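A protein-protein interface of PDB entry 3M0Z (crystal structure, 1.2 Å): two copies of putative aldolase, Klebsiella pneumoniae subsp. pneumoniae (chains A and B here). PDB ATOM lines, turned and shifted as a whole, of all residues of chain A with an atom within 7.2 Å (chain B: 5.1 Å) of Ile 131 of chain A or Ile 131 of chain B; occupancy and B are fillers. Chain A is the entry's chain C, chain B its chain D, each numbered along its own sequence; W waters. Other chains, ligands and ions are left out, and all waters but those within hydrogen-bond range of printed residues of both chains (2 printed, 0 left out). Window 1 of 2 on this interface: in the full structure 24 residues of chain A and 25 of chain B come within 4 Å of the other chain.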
ATOM      1  N   VAL A  98      -6.730   9.483 -23.425  1.00  0.00           N
ATOM      2  CA  VAL A  98      -7.407   8.645 -24.411  1.00  0.00           C
ATOM      3  C   VAL A  98      -6.776   7.260 -24.435  1.00  0.00           C
ATOM      4  O   VAL A  98      -5.726   7.029 -23.839  1.00  0.00           O
ATOM      5  CB  VAL A  98      -7.421   9.316 -25.804  1.00  0.00           C
ATOM      6  CG1 VAL A  98      -8.245  10.615 -25.737  1.00  0.00           C
ATOM      7  CG2 VAL A  98      -6.021   9.532 -26.320  1.00  0.00           C
ATOM      8  N   PHE A  99      -7.426   6.310 -25.107  1.00  0.00           N
ATOM      9  CA  PHE A  99      -7.009   4.912 -24.977  1.00  0.00           C
ATOM     10  C   PHE A  99      -5.538   4.761 -25.329  1.00  0.00           C
ATOM     11  O   PHE A  99      -4.830   4.001 -24.676  1.00  0.00           O
ATOM     12  CB  PHE A  99      -7.924   4.054 -25.868  1.00  0.00           C
ATOM     13  CG  PHE A  99      -7.591   2.601 -25.866  1.00  0.00           C
ATOM     14  CD1 PHE A  99      -8.150   1.716 -24.938  1.00  0.00           C
ATOM     15  CD2 PHE A  99      -6.708   2.089 -26.822  1.00  0.00           C
ATOM     16  CE1 PHE A  99      -7.819   0.300 -24.983  1.00  0.00           C
ATOM     17  CE2 PHE A  99      -6.382   0.731 -26.845  1.00  0.00           C
ATOM     18  CZ  PHE A  99      -6.963  -0.148 -25.940  1.00  0.00           C
ATOM     19  N   THR A 100      -5.096   5.467 -26.374  1.00  0.00           N
ATOM     20  CA  THR A 100      -3.750   5.328 -26.906  1.00  0.00           C
ATOM     21  C   THR A 100      -2.693   6.159 -26.186  1.00  0.00           C
ATOM     22  O   THR A 100      -1.540   6.136 -26.603  1.00  0.00           O
ATOM     23  CB  THR A 100      -3.754   5.732 -28.382  1.00  0.00           C
ATOM     24  OG1 THR A 100      -4.310   7.045 -28.508  1.00  0.00           O
ATOM     25  CG2 THR A 100      -4.614   4.805 -29.233  1.00  0.00           C
ATOM     26  N   LEU A 119     -10.045   6.764 -21.893  1.00  0.00           N
ATOM     27  CA  LEU A 119     -11.356   7.055 -22.496  1.00  0.00           C
ATOM     28  C   LEU A 119     -11.784   5.939 -23.438  1.00  0.00           C
ATOM     29  O   LEU A 119     -11.105   5.644 -24.439  1.00  0.00           O
ATOM     30  CB  LEU A 119     -11.209   8.381 -23.254  1.00  0.00           C
ATOM     31  CG  LEU A 119     -12.504   9.135 -23.580  1.00  0.00           C
ATOM     32  CD1 LEU A 119     -12.214  10.616 -23.881  1.00  0.00           C
ATOM     33  CD2 LEU A 119     -13.275   8.513 -24.690  1.00  0.00           C
ATOM     34  N   VAL A 120     -12.935   5.339 -23.111  1.00  0.00           N
ATOM     35  CA  VAL A 120     -13.628   4.386 -23.972  1.00  0.00           C
ATOM     36  C   VAL A 120     -15.084   4.802 -23.989  1.00  0.00           C
ATOM     37  O   VAL A 120     -15.556   5.446 -23.048  1.00  0.00           O
ATOM     38  CB  VAL A 120     -13.452   2.918 -23.519  1.00  0.00           C
ATOM     39  CG1 VAL A 120     -11.962   2.569 -23.343  1.00  0.00           C
ATOM     40  CG2 VAL A 120     -14.231   2.635 -22.254  1.00  0.00           C
ATOM     41  N   SER A 121     -15.793   4.441 -25.060  1.00  0.00           N
ATOM     42  CA  SER A 121     -17.047   5.131 -25.336  1.00  0.00           C
ATOM     43  C   SER A 121     -18.221   4.176 -25.611  1.00  0.00           C
ATOM     44  O   SER A 121     -18.028   3.038 -26.053  1.00  0.00           O
ATOM     45  CB  SER A 121     -16.895   6.063 -26.532  1.00  0.00           C
ATOM     46  OG  SER A 121     -15.846   6.990 -26.306  1.00  0.00           O
ATOM     47  N   THR A 123     -21.399   2.459 -27.526  1.00  0.00           N
ATOM     48  CA  THR A 123     -21.528   1.947 -28.868  1.00  0.00           C
ATOM     49  C   THR A 123     -22.987   1.746 -29.306  1.00  0.00           C
ATOM     50  O   THR A 123     -23.239   1.483 -30.473  1.00  0.00           O
ATOM     51  CB  THR A 123     -20.894   0.558 -28.968  1.00  0.00           C
ATOM     52  OG1 THR A 123     -21.527  -0.308 -28.027  1.00  0.00           O
ATOM     53  CG2 THR A 123     -19.365   0.624 -28.765  1.00  0.00           C
ATOM     54  N   VAL A 129     -17.592  -1.693 -26.007  1.00  0.00           N
ATOM     55  CA  VAL A 129     -17.154  -0.311 -25.959  1.00  0.00           C
ATOM     56  C   VAL A 129     -16.192  -0.004 -27.091  1.00  0.00           C
ATOM     57  O   VAL A 129     -15.437  -0.877 -27.568  1.00  0.00           O
ATOM     58  CB  VAL A 129     -16.492   0.060 -24.580  1.00  0.00           C
ATOM     59  CG1 VAL A 129     -17.537   0.133 -23.464  1.00  0.00           C
ATOM     60  CG2 VAL A 129     -15.332  -0.883 -24.235  1.00  0.00           C
ATOM     61  N   LYS A 130     -16.211   1.253 -27.522  1.00  0.00           N
ATOM     62  CA  LYS A 130     -15.310   1.729 -28.562  1.00  0.00           C
ATOM     63  C   LYS A 130     -14.000   2.196 -27.906  1.00  0.00           C
ATOM     64  O   LYS A 130     -14.017   3.067 -27.016  1.00  0.00           O
ATOM     65  CB  LYS A 130     -16.011   2.864 -29.316  1.00  0.00           C
ATOM     66  CG  LYS A 130     -15.099   3.700 -30.196  1.00  0.00           C
ATOM     67  CD  LYS A 130     -15.865   4.704 -31.098  1.00  0.00           C
ATOM     68  CE  LYS A 130     -14.946   5.710 -31.710  1.00  0.00           C
ATOM     69  NZ  LYS A 130     -15.720   6.524 -32.682  1.00  0.00           N
ATOM     70  N   ILE A 131     -12.876   1.592 -28.360  1.00  0.00           N
ATOM     71  CA  ILE A 131     -11.540   1.904 -27.852  1.00  0.00           C
ATOM     72  C   ILE A 131     -10.709   2.779 -28.792  1.00  0.00           C
ATOM     73  O   ILE A 131      -9.643   3.236 -28.402  1.00  0.00           O
ATOM     74  CB  ILE A 131     -10.714   0.619 -27.544  1.00  0.00           C
ATOM     75  CG1 ILE A 131     -10.458  -0.221 -28.804  1.00  0.00           C
ATOM     76  CG2 ILE A 131     -11.383  -0.196 -26.446  1.00  0.00           C
ATOM     77  CD1 ILE A 131      -9.491  -1.360 -28.573  1.00  0.00           C
ATOM     78  N   SER A 132     -11.197   3.027 -30.003  1.00  0.00           N
ATOM     79  CA  SER A 132     -10.434   3.767 -30.988  1.00  0.00           C
ATOM     80  C   SER A 132     -10.584   5.270 -30.778  1.00  0.00           C
ATOM     81  O   SER A 132     -11.166   5.987 -31.598  1.00  0.00           O
ATOM     82  CB  SER A 132     -10.870   3.322 -32.368  1.00  0.00           C
ATOM     83  OG  SER A 132     -12.283   3.322 -32.521  1.00  0.00           O
ATOM     84  N   THR A 133     -10.029   5.748 -29.661  1.00  0.00           N
ATOM     85  CA  THR A 133     -10.281   7.121 -29.218  1.00  0.00           C
ATOM     86  C   THR A 133      -9.040   8.012 -29.244  1.00  0.00           C
ATOM     87  O   THR A 133      -9.062   9.125 -28.732  1.00  0.00           O
ATOM     88  CB  THR A 133     -10.900   7.110 -27.799  1.00  0.00           C
ATOM     89  OG1 THR A 133      -9.978   6.484 -26.892  1.00  0.00           O
ATOM     90  CG2 THR A 133     -12.216   6.343 -27.783  1.00  0.00           C
ATOM     91  N   GLY A 134      -7.983   7.534 -29.900  1.00  0.00           N
ATOM     92  CA  GLY A 134      -6.764   8.324 -30.066  1.00  0.00           C
ATOM     93  C   GLY A 134      -6.780   9.237 -31.275  1.00  0.00           C
ATOM     94  O   GLY A 134      -7.751   9.288 -32.009  1.00  0.00           O
ATOM     95  N   SER A 137      -6.690   6.989 -34.488  1.00  0.00           N
ATOM     96  CA  SER A 137      -7.666   5.913 -34.372  1.00  0.00           C
ATOM     97  C   SER A 137      -9.085   6.446 -34.292  1.00  0.00           C
ATOM     98  O   SER A 137      -9.992   5.774 -34.799  1.00  0.00           O
ATOM     99  CB  SER A 137      -7.317   4.964 -33.208  1.00  0.00           C
ATOM    100  OG  SER A 137      -7.143   5.667 -31.987  1.00  0.00           O
ATOM    101  N   SER A 138      -9.295   7.645 -33.753  1.00  0.00           N
ATOM    102  CA  SER A 138     -10.643   8.243 -33.754  1.00  0.00           C
ATOM    103  C   SER A 138     -11.170   8.553 -35.135  1.00  0.00           C
ATOM    104  O   SER A 138     -12.385   8.685 -35.294  1.00  0.00           O
ATOM    105  CB  SER A 138     -10.673   9.478 -32.897  1.00  0.00           C
ATOM    106  OG  SER A 138      -9.847  10.518 -33.411  1.00  0.00           O
ATOM    107  N   ASP A 142     -14.495   2.352 -36.427  1.00  0.00           N
ATOM    108  CA  ASP A 142     -14.498   2.087 -35.002  1.00  0.00           C
ATOM    109  C   ASP A 142     -13.878   0.726 -34.650  1.00  0.00           C
ATOM    110  O   ASP A 142     -14.154  -0.288 -35.301  1.00  0.00           O
ATOM    111  CB  ASP A 142     -15.929   2.115 -34.458  1.00  0.00           C
ATOM    112  CG  ASP A 142     -16.586   3.473 -34.548  1.00  0.00           C
ATOM    113  OD1 ASP A 142     -15.892   4.481 -34.776  1.00  0.00           O
ATOM    114  OD2 ASP A 142     -17.823   3.504 -34.362  1.00  0.00           O
ATOM    115  N   GLY A 143     -13.096   0.736 -33.571  1.00  0.00           N
ATOM    116  CA  GLY A 143     -12.653  -0.500 -32.964  1.00  0.00           C
ATOM    117  C   GLY A 143     -13.430  -0.734 -31.694  1.00  0.00           C
ATOM    118  O   GLY A 143     -13.364   0.083 -30.746  1.00  0.00           O
ATOM    119  N   ILE A 144     -14.170  -1.850 -31.678  1.00  0.00           N
ATOM    120  CA  ILE A 144     -15.178  -2.124 -30.657  1.00  0.00           C
ATOM    121  C   ILE A 144     -14.871  -3.467 -30.051  1.00  0.00           C
ATOM    122  O   ILE A 144     -14.717  -4.459 -30.793  1.00  0.00           O
ATOM    123  CB  ILE A 144     -16.594  -2.077 -31.308  1.00  0.00           C
ATOM    124  CG1 ILE A 144     -16.916  -0.630 -31.733  1.00  0.00           C
ATOM    125  CG2 ILE A 144     -17.656  -2.582 -30.336  1.00  0.00           C
ATOM    126  CD1 ILE A 144     -18.095  -0.529 -32.765  1.00  0.00           C
ATOM    127  N   VAL A 145     -14.747  -3.518 -28.712  1.00  0.00           N
ATOM    128  CA  VAL A 145     -14.333  -4.741 -28.023  1.00  0.00           C
ATOM    129  C   VAL A 145     -15.212  -4.959 -26.785  1.00  0.00           C
ATOM    130  O   VAL A 145     -15.831  -4.034 -26.268  1.00  0.00           O
ATOM    131  CB  VAL A 145     -12.820  -4.701 -27.606  1.00  0.00           C
ATOM    132  CG1 VAL A 145     -11.969  -4.412 -28.792  1.00  0.00           C
ATOM    133  CG2 VAL A 145     -12.572  -3.672 -26.501  1.00  0.00           C
ATOM    134  N   PRO A 146     -15.232  -6.196 -26.253  1.00  0.00           N
ATOM    135  CA  PRO A 146     -15.981  -6.441 -25.027  1.00  0.00           C
ATOM    136  C   PRO A 146     -15.404  -5.667 -23.842  1.00  0.00           C
ATOM    137  O   PRO A 146     -14.193  -5.427 -23.772  1.00  0.00           O
ATOM    138  CB  PRO A 146     -15.784  -7.935 -24.790  1.00  0.00           C
ATOM    139  CG  PRO A 146     -15.508  -8.520 -26.196  1.00  0.00           C
ATOM    140  CD  PRO A 146     -14.644  -7.428 -26.806  1.00  0.00           C
ATOM    141  N   THR A 149     -12.375  -7.100 -22.080  1.00  0.00           N
ATOM    142  CA  THR A 149     -11.167  -6.928 -22.886  1.00  0.00           C
ATOM    143  C   THR A 149     -10.655  -5.493 -22.781  1.00  0.00           C
ATOM    144  O   THR A 149      -9.457  -5.283 -22.664  1.00  0.00           O
ATOM    145  CB  THR A 149     -11.494  -7.272 -24.364  1.00  0.00           C
ATOM    146  OG1 THR A 149     -12.297  -8.458 -24.391  1.00  0.00           O
ATOM    147  CG2 THR A 149     -10.212  -7.477 -25.163  1.00  0.00           C
ATOM    148  N   ALA A 150     -11.560  -4.509 -22.841  1.00  0.00           N
ATOM    149  CA  ALA A 150     -11.151  -3.121 -22.683  1.00  0.00           C
ATOM    150  C   ALA A 150     -10.468  -2.935 -21.327  1.00  0.00           C
ATOM    151  O   ALA A 150      -9.468  -2.224 -21.219  1.00  0.00           O
ATOM    152  CB  ALA A 150     -12.367  -2.193 -22.847  1.00  0.00           C
ATOM    153  N   ILE A 151     -11.042  -3.513 -20.263  1.00  0.00           N
ATOM    154  CA  ILE A 151     -10.456  -3.414 -18.927  1.00  0.00           C
ATOM    155  C   ILE A 151      -9.064  -4.033 -18.911  1.00  0.00           C
ATOM    156  O   ILE A 151      -8.110  -3.428 -18.395  1.00  0.00           O
ATOM    157  CB  ILE A 151     -11.391  -4.076 -17.899  1.00  0.00           C
ATOM    158  CG1 ILE A 151     -12.621  -3.191 -17.717  1.00  0.00           C
ATOM    159  CG2 ILE A 151     -10.654  -4.303 -16.560  1.00  0.00           C
ATOM    160  CD1 ILE A 151     -13.833  -3.861 -16.977  1.00  0.00           C
ATOM    161  N   LEU A 153      -6.999  -4.623 -21.412  1.00  0.00           N
ATOM    162  CA  LEU A 153      -6.095  -3.785 -22.229  1.00  0.00           C
ATOM    163  C   LEU A 153      -5.624  -2.579 -21.430  1.00  0.00           C
ATOM    164  O   LEU A 153      -4.414  -2.261 -21.403  1.00  0.00           O
ATOM    165  CB  LEU A 153      -6.835  -3.313 -23.479  1.00  0.00           C
ATOM    166  CG  LEU A 153      -7.012  -4.371 -24.583  1.00  0.00           C
ATOM    167  CD1 LEU A 153      -8.104  -3.979 -25.564  1.00  0.00           C
ATOM    168  CD2 LEU A 153      -5.695  -4.662 -25.304  1.00  0.00           C
ATOM    169  N   LEU A 154      -6.560  -1.873 -20.792  1.00  0.00           N
ATOM    170  CA  LEU A 154      -6.185  -0.682 -20.014  1.00  0.00           C
ATOM    171  C   LEU A 154      -5.258  -1.053 -18.852  1.00  0.00           C
ATOM    172  O   LEU A 154      -4.278  -0.345 -18.613  1.00  0.00           O
ATOM    173  CB  LEU A 154      -7.442   0.048 -19.538  1.00  0.00           C
ATOM    174  CG  LEU A 154      -8.184   0.811 -20.638  1.00  0.00           C
ATOM    175  CD1 LEU A 154      -9.543   1.231 -20.113  1.00  0.00           C
ATOM    176  CD2 LEU A 154      -7.395   2.016 -21.147  1.00  0.00           C
ATOM    177  N   PHE B  99       0.710  -5.796 -28.099  1.00  0.00           N
ATOM    178  CA  PHE B  99      -0.060  -4.583 -28.444  1.00  0.00           C
ATOM    179  C   PHE B  99      -0.004  -3.534 -27.324  1.00  0.00           C
ATOM    180  O   PHE B  99       0.110  -2.337 -27.569  1.00  0.00           O
ATOM    181  CB  PHE B  99      -1.485  -4.994 -28.780  1.00  0.00           C
ATOM    182  CG  PHE B  99      -2.419  -3.844 -29.106  1.00  0.00           C
ATOM    183  CD1 PHE B  99      -2.575  -3.367 -30.425  1.00  0.00           C
ATOM    184  CD2 PHE B  99      -3.168  -3.263 -28.097  1.00  0.00           C
ATOM    185  CE1 PHE B  99      -3.477  -2.290 -30.678  1.00  0.00           C
ATOM    186  CE2 PHE B  99      -4.048  -2.225 -28.330  1.00  0.00           C
ATOM    187  CZ  PHE B  99      -4.193  -1.739 -29.627  1.00  0.00           C
ATOM    188  N   LEU B 119       2.355  -6.825 -31.716  1.00  0.00           N
ATOM    189  CA  LEU B 119       1.837  -8.137 -32.097  1.00  0.00           C
ATOM    190  C   LEU B 119       0.311  -8.071 -32.185  1.00  0.00           C
ATOM    191  O   LEU B 119      -0.360  -7.644 -31.229  1.00  0.00           O
ATOM    192  CB  LEU B 119       2.295  -9.143 -31.052  1.00  0.00           C
ATOM    193  CG  LEU B 119       2.239 -10.621 -31.402  1.00  0.00           C
ATOM    194  CD1 LEU B 119       3.144 -11.381 -30.450  1.00  0.00           C
ATOM    195  CD2 LEU B 119       0.797 -11.165 -31.415  1.00  0.00           C
ATOM    196  N   VAL B 120      -0.235  -8.431 -33.357  1.00  0.00           N
ATOM    197  CA  VAL B 120      -1.677  -8.611 -33.581  1.00  0.00           C
ATOM    198  C   VAL B 120      -1.857  -9.922 -34.327  1.00  0.00           C
ATOM    199  O   VAL B 120      -0.903 -10.413 -34.972  1.00  0.00           O
ATOM    200  CB  VAL B 120      -2.332  -7.423 -34.307  1.00  0.00           C
ATOM    201  CG1 VAL B 120      -2.018  -6.104 -33.588  1.00  0.00           C
ATOM    202  CG2 VAL B 120      -1.971  -7.379 -35.745  1.00  0.00           C
ATOM    203  N   VAL B 129      -8.409  -8.161 -37.109  1.00  0.00           N
ATOM    204  CA  VAL B 129      -7.279  -8.695 -36.346  1.00  0.00           C
ATOM    205  C   VAL B 129      -7.527  -8.596 -34.852  1.00  0.00           C
ATOM    206  O   VAL B 129      -8.245  -7.706 -34.367  1.00  0.00           O
ATOM    207  CB  VAL B 129      -5.941  -7.990 -36.700  1.00  0.00           C
ATOM    208  CG1 VAL B 129      -5.523  -8.385 -38.112  1.00  0.00           C
ATOM    209  CG2 VAL B 129      -6.011  -6.461 -36.520  1.00  0.00           C
ATOM    210  N   LYS B 130      -6.924  -9.540 -34.149  1.00  0.00           N
ATOM    211  CA  LYS B 130      -7.003  -9.587 -32.692  1.00  0.00           C
ATOM    212  C   LYS B 130      -5.893  -8.743 -32.069  1.00  0.00           C
ATOM    213  O   LYS B 130      -4.725  -8.965 -32.378  1.00  0.00           O
ATOM    214  CB  LYS B 130      -6.911 -11.051 -32.218  1.00  0.00           C
ATOM    215  CG  LYS B 130      -6.705 -11.219 -30.702  1.00  0.00           C
ATOM    216  CD  LYS B 130      -6.826 -12.690 -30.340  1.00  0.00           C
ATOM    217  CE  LYS B 130      -6.142 -12.965 -29.000  1.00  0.00           C
ATOM    218  NZ  LYS B 130      -6.484 -14.342 -28.495  1.00  0.00           N
ATOM    219  N   ILE B 131      -6.296  -7.780 -31.241  1.00  0.00           N
ATOM    220  CA  ILE B 131      -5.384  -6.849 -30.596  1.00  0.00           C
ATOM    221  C   ILE B 131      -5.137  -7.134 -29.119  1.00  0.00           C
ATOM    222  O   ILE B 131      -4.283  -6.499 -28.492  1.00  0.00           O
ATOM    223  CB  ILE B 131      -5.834  -5.370 -30.738  1.00  0.00           C
ATOM    224  CG1 ILE B 131      -7.186  -5.084 -30.055  1.00  0.00           C
ATOM    225  CG2 ILE B 131      -5.769  -4.913 -32.193  1.00  0.00           C
ATOM    226  CD1 ILE B 131      -7.522  -3.613 -29.987  1.00  0.00           C
ATOM    227  N   SER B 132      -5.861  -8.101 -28.562  1.00  0.00           N
ATOM    228  CA  SER B 132      -5.794  -8.383 -27.156  1.00  0.00           C
ATOM    229  C   SER B 132      -4.665  -9.338 -26.825  1.00  0.00           C
ATOM    230  O   SER B 132      -4.882 -10.483 -26.444  1.00  0.00           O
ATOM    231  CB  SER B 132      -7.150  -8.860 -26.655  1.00  0.00           C
ATOM    232  OG  SER B 132      -7.632  -9.882 -27.520  1.00  0.00           O
ATOM    233  N   THR B 133      -3.441  -8.844 -26.986  1.00  0.00           N
ATOM    234  CA  THR B 133      -2.247  -9.714 -26.975  1.00  0.00           C
ATOM    235  C   THR B 133      -1.319  -9.417 -25.799  1.00  0.00           C
ATOM    236  O   THR B 133      -0.208  -9.935 -25.753  1.00  0.00           O
ATOM    237  CB  THR B 133      -1.489  -9.650 -28.324  1.00  0.00           C
ATOM    238  OG1 THR B 133      -1.035  -8.296 -28.539  1.00  0.00           O
ATOM    239  CG2 THR B 133      -2.408 -10.139 -29.464  1.00  0.00           C
ATOM    240  N   GLY B 134      -1.754  -8.587 -24.850  1.00  0.00           N
ATOM    241  CA  GLY B 134      -0.938  -8.262 -23.656  1.00  0.00           C
ATOM    242  C   GLY B 134      -1.099  -9.272 -22.529  1.00  0.00           C
ATOM    243  O   GLY B 134      -1.816 -10.278 -22.650  1.00  0.00           O
ATOM    244  N   SER B 137      -4.780  -9.049 -21.202  1.00  0.00           N
ATOM    245  CA  SER B 137      -5.726  -9.025 -22.300  1.00  0.00           C
ATOM    246  C   SER B 137      -5.701 -10.306 -23.125  1.00  0.00           C
ATOM    247  O   SER B 137      -6.731 -10.708 -23.635  1.00  0.00           O
ATOM    248  CB  SER B 137      -5.531  -7.760 -23.136  1.00  0.00           C
ATOM    249  OG  SER B 137      -4.196  -7.606 -23.619  1.00  0.00           O
ATOM    250  N   GLY B 143     -10.365  -9.223 -28.320  1.00  0.00           N
ATOM    251  CA  GLY B 143     -10.671  -7.870 -28.843  1.00  0.00           C
ATOM    252  C   GLY B 143     -10.235  -7.790 -30.281  1.00  0.00           C
ATOM    253  O   GLY B 143      -9.047  -7.966 -30.600  1.00  0.00           O
ATOM    254  N   ILE B 144     -11.225  -7.629 -31.162  1.00  0.00           N
ATOM    255  CA  ILE B 144     -11.027  -7.727 -32.610  1.00  0.00           C
ATOM    256  C   ILE B 144     -11.452  -6.443 -33.280  1.00  0.00           C
ATOM    257  O   ILE B 144     -12.552  -5.937 -33.012  1.00  0.00           O
ATOM    258  CB  ILE B 144     -11.834  -8.942 -33.158  1.00  0.00           C
ATOM    259  CG1 ILE B 144     -11.265 -10.236 -32.555  1.00  0.00           C
ATOM    260  CG2 ILE B 144     -11.784  -8.972 -34.680  1.00  0.00           C
ATOM    261  CD1 ILE B 144     -12.122 -11.464 -32.777  1.00  0.00           C
ATOM    262  N   VAL B 145     -10.560  -5.875 -34.105  1.00  0.00           N
ATOM    263  CA  VAL B 145     -10.830  -4.599 -34.742  1.00  0.00           C
ATOM    264  C   VAL B 145     -10.444  -4.683 -36.229  1.00  0.00           C
ATOM    265  O   VAL B 145      -9.648  -5.554 -36.619  1.00  0.00           O
ATOM    266  CB  VAL B 145     -10.096  -3.427 -34.032  1.00  0.00           C
ATOM    267  CG1 VAL B 145     -10.463  -3.356 -32.552  1.00  0.00           C
ATOM    268  CG2 VAL B 145      -8.542  -3.539 -34.242  1.00  0.00           C
ATOM    269  N   ALA B 150      -6.513  -1.109 -36.259  1.00  0.00           N
ATOM    270  CA  ALA B 150      -5.326  -1.635 -35.582  1.00  0.00           C
ATOM    271  C   ALA B 150      -4.099  -0.822 -35.955  1.00  0.00           C
ATOM    272  O   ALA B 150      -3.277  -0.484 -35.087  1.00  0.00           O
ATOM    273  CB  ALA B 150      -5.154  -3.094 -35.925  1.00  0.00           C
ATOM    274  N   LEU B 153      -4.337   2.632 -34.277  1.00  0.00           N
ATOM    275  CA  LEU B 153      -4.069   2.459 -32.853  1.00  0.00           C
ATOM    276  C   LEU B 153      -2.563   2.324 -32.623  1.00  0.00           C
ATOM    277  O   LEU B 153      -1.978   2.953 -31.716  1.00  0.00           O
ATOM    278  CB  LEU B 153      -4.805   1.234 -32.306  1.00  0.00           C
ATOM    279  CG  LEU B 153      -6.308   1.402 -32.079  1.00  0.00           C
ATOM    280  CD1 LEU B 153      -6.993   0.031 -31.966  1.00  0.00           C
ATOM    281  CD2 LEU B 153      -6.588   2.227 -30.840  1.00  0.00           C
HETATM  282  O   HOH W   1     -13.896  -7.196 -30.300  1.00  0.00           O
HETATM  283  O   HOH W   2     -14.074  -3.620 -33.913  1.00  0.00           O
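Printed residues of chain B within 4 Å of Thr 100 of chain A: Leu 153 (3.6 Å).
Ser 121 of chain A touches none of the printed residues of chain B.
Printed residues of chain B within 4 Å of Ile 131 of chain A: Ile 131 (3.3 Å).
Ser 132 of chain A touches none of the printed residues of chain B.
Of the printed residues of chain B, Ser 137 of chain A touches Leu 153 (3.7 Å).
Of the printed residues of chain B, Ile 144 of chain A touches Ile 144 (3.4 Å).
Of the printed residues of chain B, Val 145 of chain A touches Gly 143.
Of the printed residues of chain A, Ile 131 of chain B touches Ile 131 and Leu 153.
Of the printed residues of chain A, Val 145 of chain B touches Gly 143.
The nearest printed residue of chain B that does not touch Val 145 of chain A is Ile 144 of chain B (4.1 Å).
Thr 100 of chain A touches Leu 153 of chain B.
Ile 131 of chain A touches Ile 131 of chain B (CD1 to CD1, 3.3 Å).
CD2 of Leu 153 of chain B touches OG of Ser 137 of chain A (3.7 Å).
CG1 of Val 145 of chain B touches CA of Gly 143 of chain A, 3.6 Å away.
Val 145 of chain A touches Gly 143 of chain B (CG1 to CA, 3.7 Å).
Ser 132 of chain B touches Thr 149 of chain A.
CG2 of Thr 149 of chain A touches N of Gly 143 of chain B, 3.6 Å away.
Leu 153 of chain A touches Ile 131 of chain B (CD2 to O, 3.9 Å).
Leu 153 of chain A touches Ser 137 of chain B.
N of Val 129 of chain A lies within hydrogen-bond range of O of Val 145 of chain A, at 2.9 Å.
N of Val 129 of chain B sits at hydrogen-bond distance from O of Val 145 of chain B (2.9 Å).
N of Gly 134 of chain A is in hydrogen-bond range of OG of Ser 137 of chain A, at 2.9 Å.
The backbone carbonyl oxygen of Gly 143 of chain A is in hydrogen-bond range of the backbone NH of Ile 131 of chain A.
The side-chain hydroxyl (OG) of Ser 137 of chain B is in hydrogen-bond range of the backbone NH (N) of Gly 134 of chain B.
OG of Ser 132 of chain A sits at hydrogen-bond distance from N of Gly 143 of chain A, 2.9 Å away.
Water W1 lies within hydrogen-bond range of N of Ile 144 of chain B and O of Ile 144 of chain A.
Water W2 lies within hydrogen-bond range of N of Ile 144 of chain A (2.9 Å) and O of Ile 144 of chain B (2.9 Å).
O of Ile 144 of chain A lies close to O of Ile 144 of chain B (3.4 Å).
Along chain B the printed residues that touch a printed residue of chain A span positions 131 to 153.
Hydrophobic or aromatic side chains of chain A that line the printed part of chain B: Ile 131, Val 145 and Leu 153.
Among the printed residues, no Asp or Glu carboxylate lies within 4 Å of a Lys or Arg side-chain nitrogen of the other chain.
Ile 131 of chain A touches its own counterpart, Ile 131 of chain B.
Ser 137 of chain A touches Leu 153 of chain B, and with the chains exchanged Leu 153 of chain A touches Ser 137 of chain B.
Gly 143 of chain A touches Val 145 of chain B, and with the chains exchanged Val 145 of chain A touches Gly 143 of chain B.
Leu 153 of chain A touches Ile 131 of chain B, but with the chains exchanged Ile 131 of chain A does not touch Leu 153 of chain B (4.04 Å).
Positions printed for both chains: 99, 119, 120, 129, 130, 131, 132, 133, 134, 137, 143, 144, 145, 150 and 153.
Of the 10 pairs that touch across the chains among the printed residues, 6 have their exchanged pair printed and touching as well.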
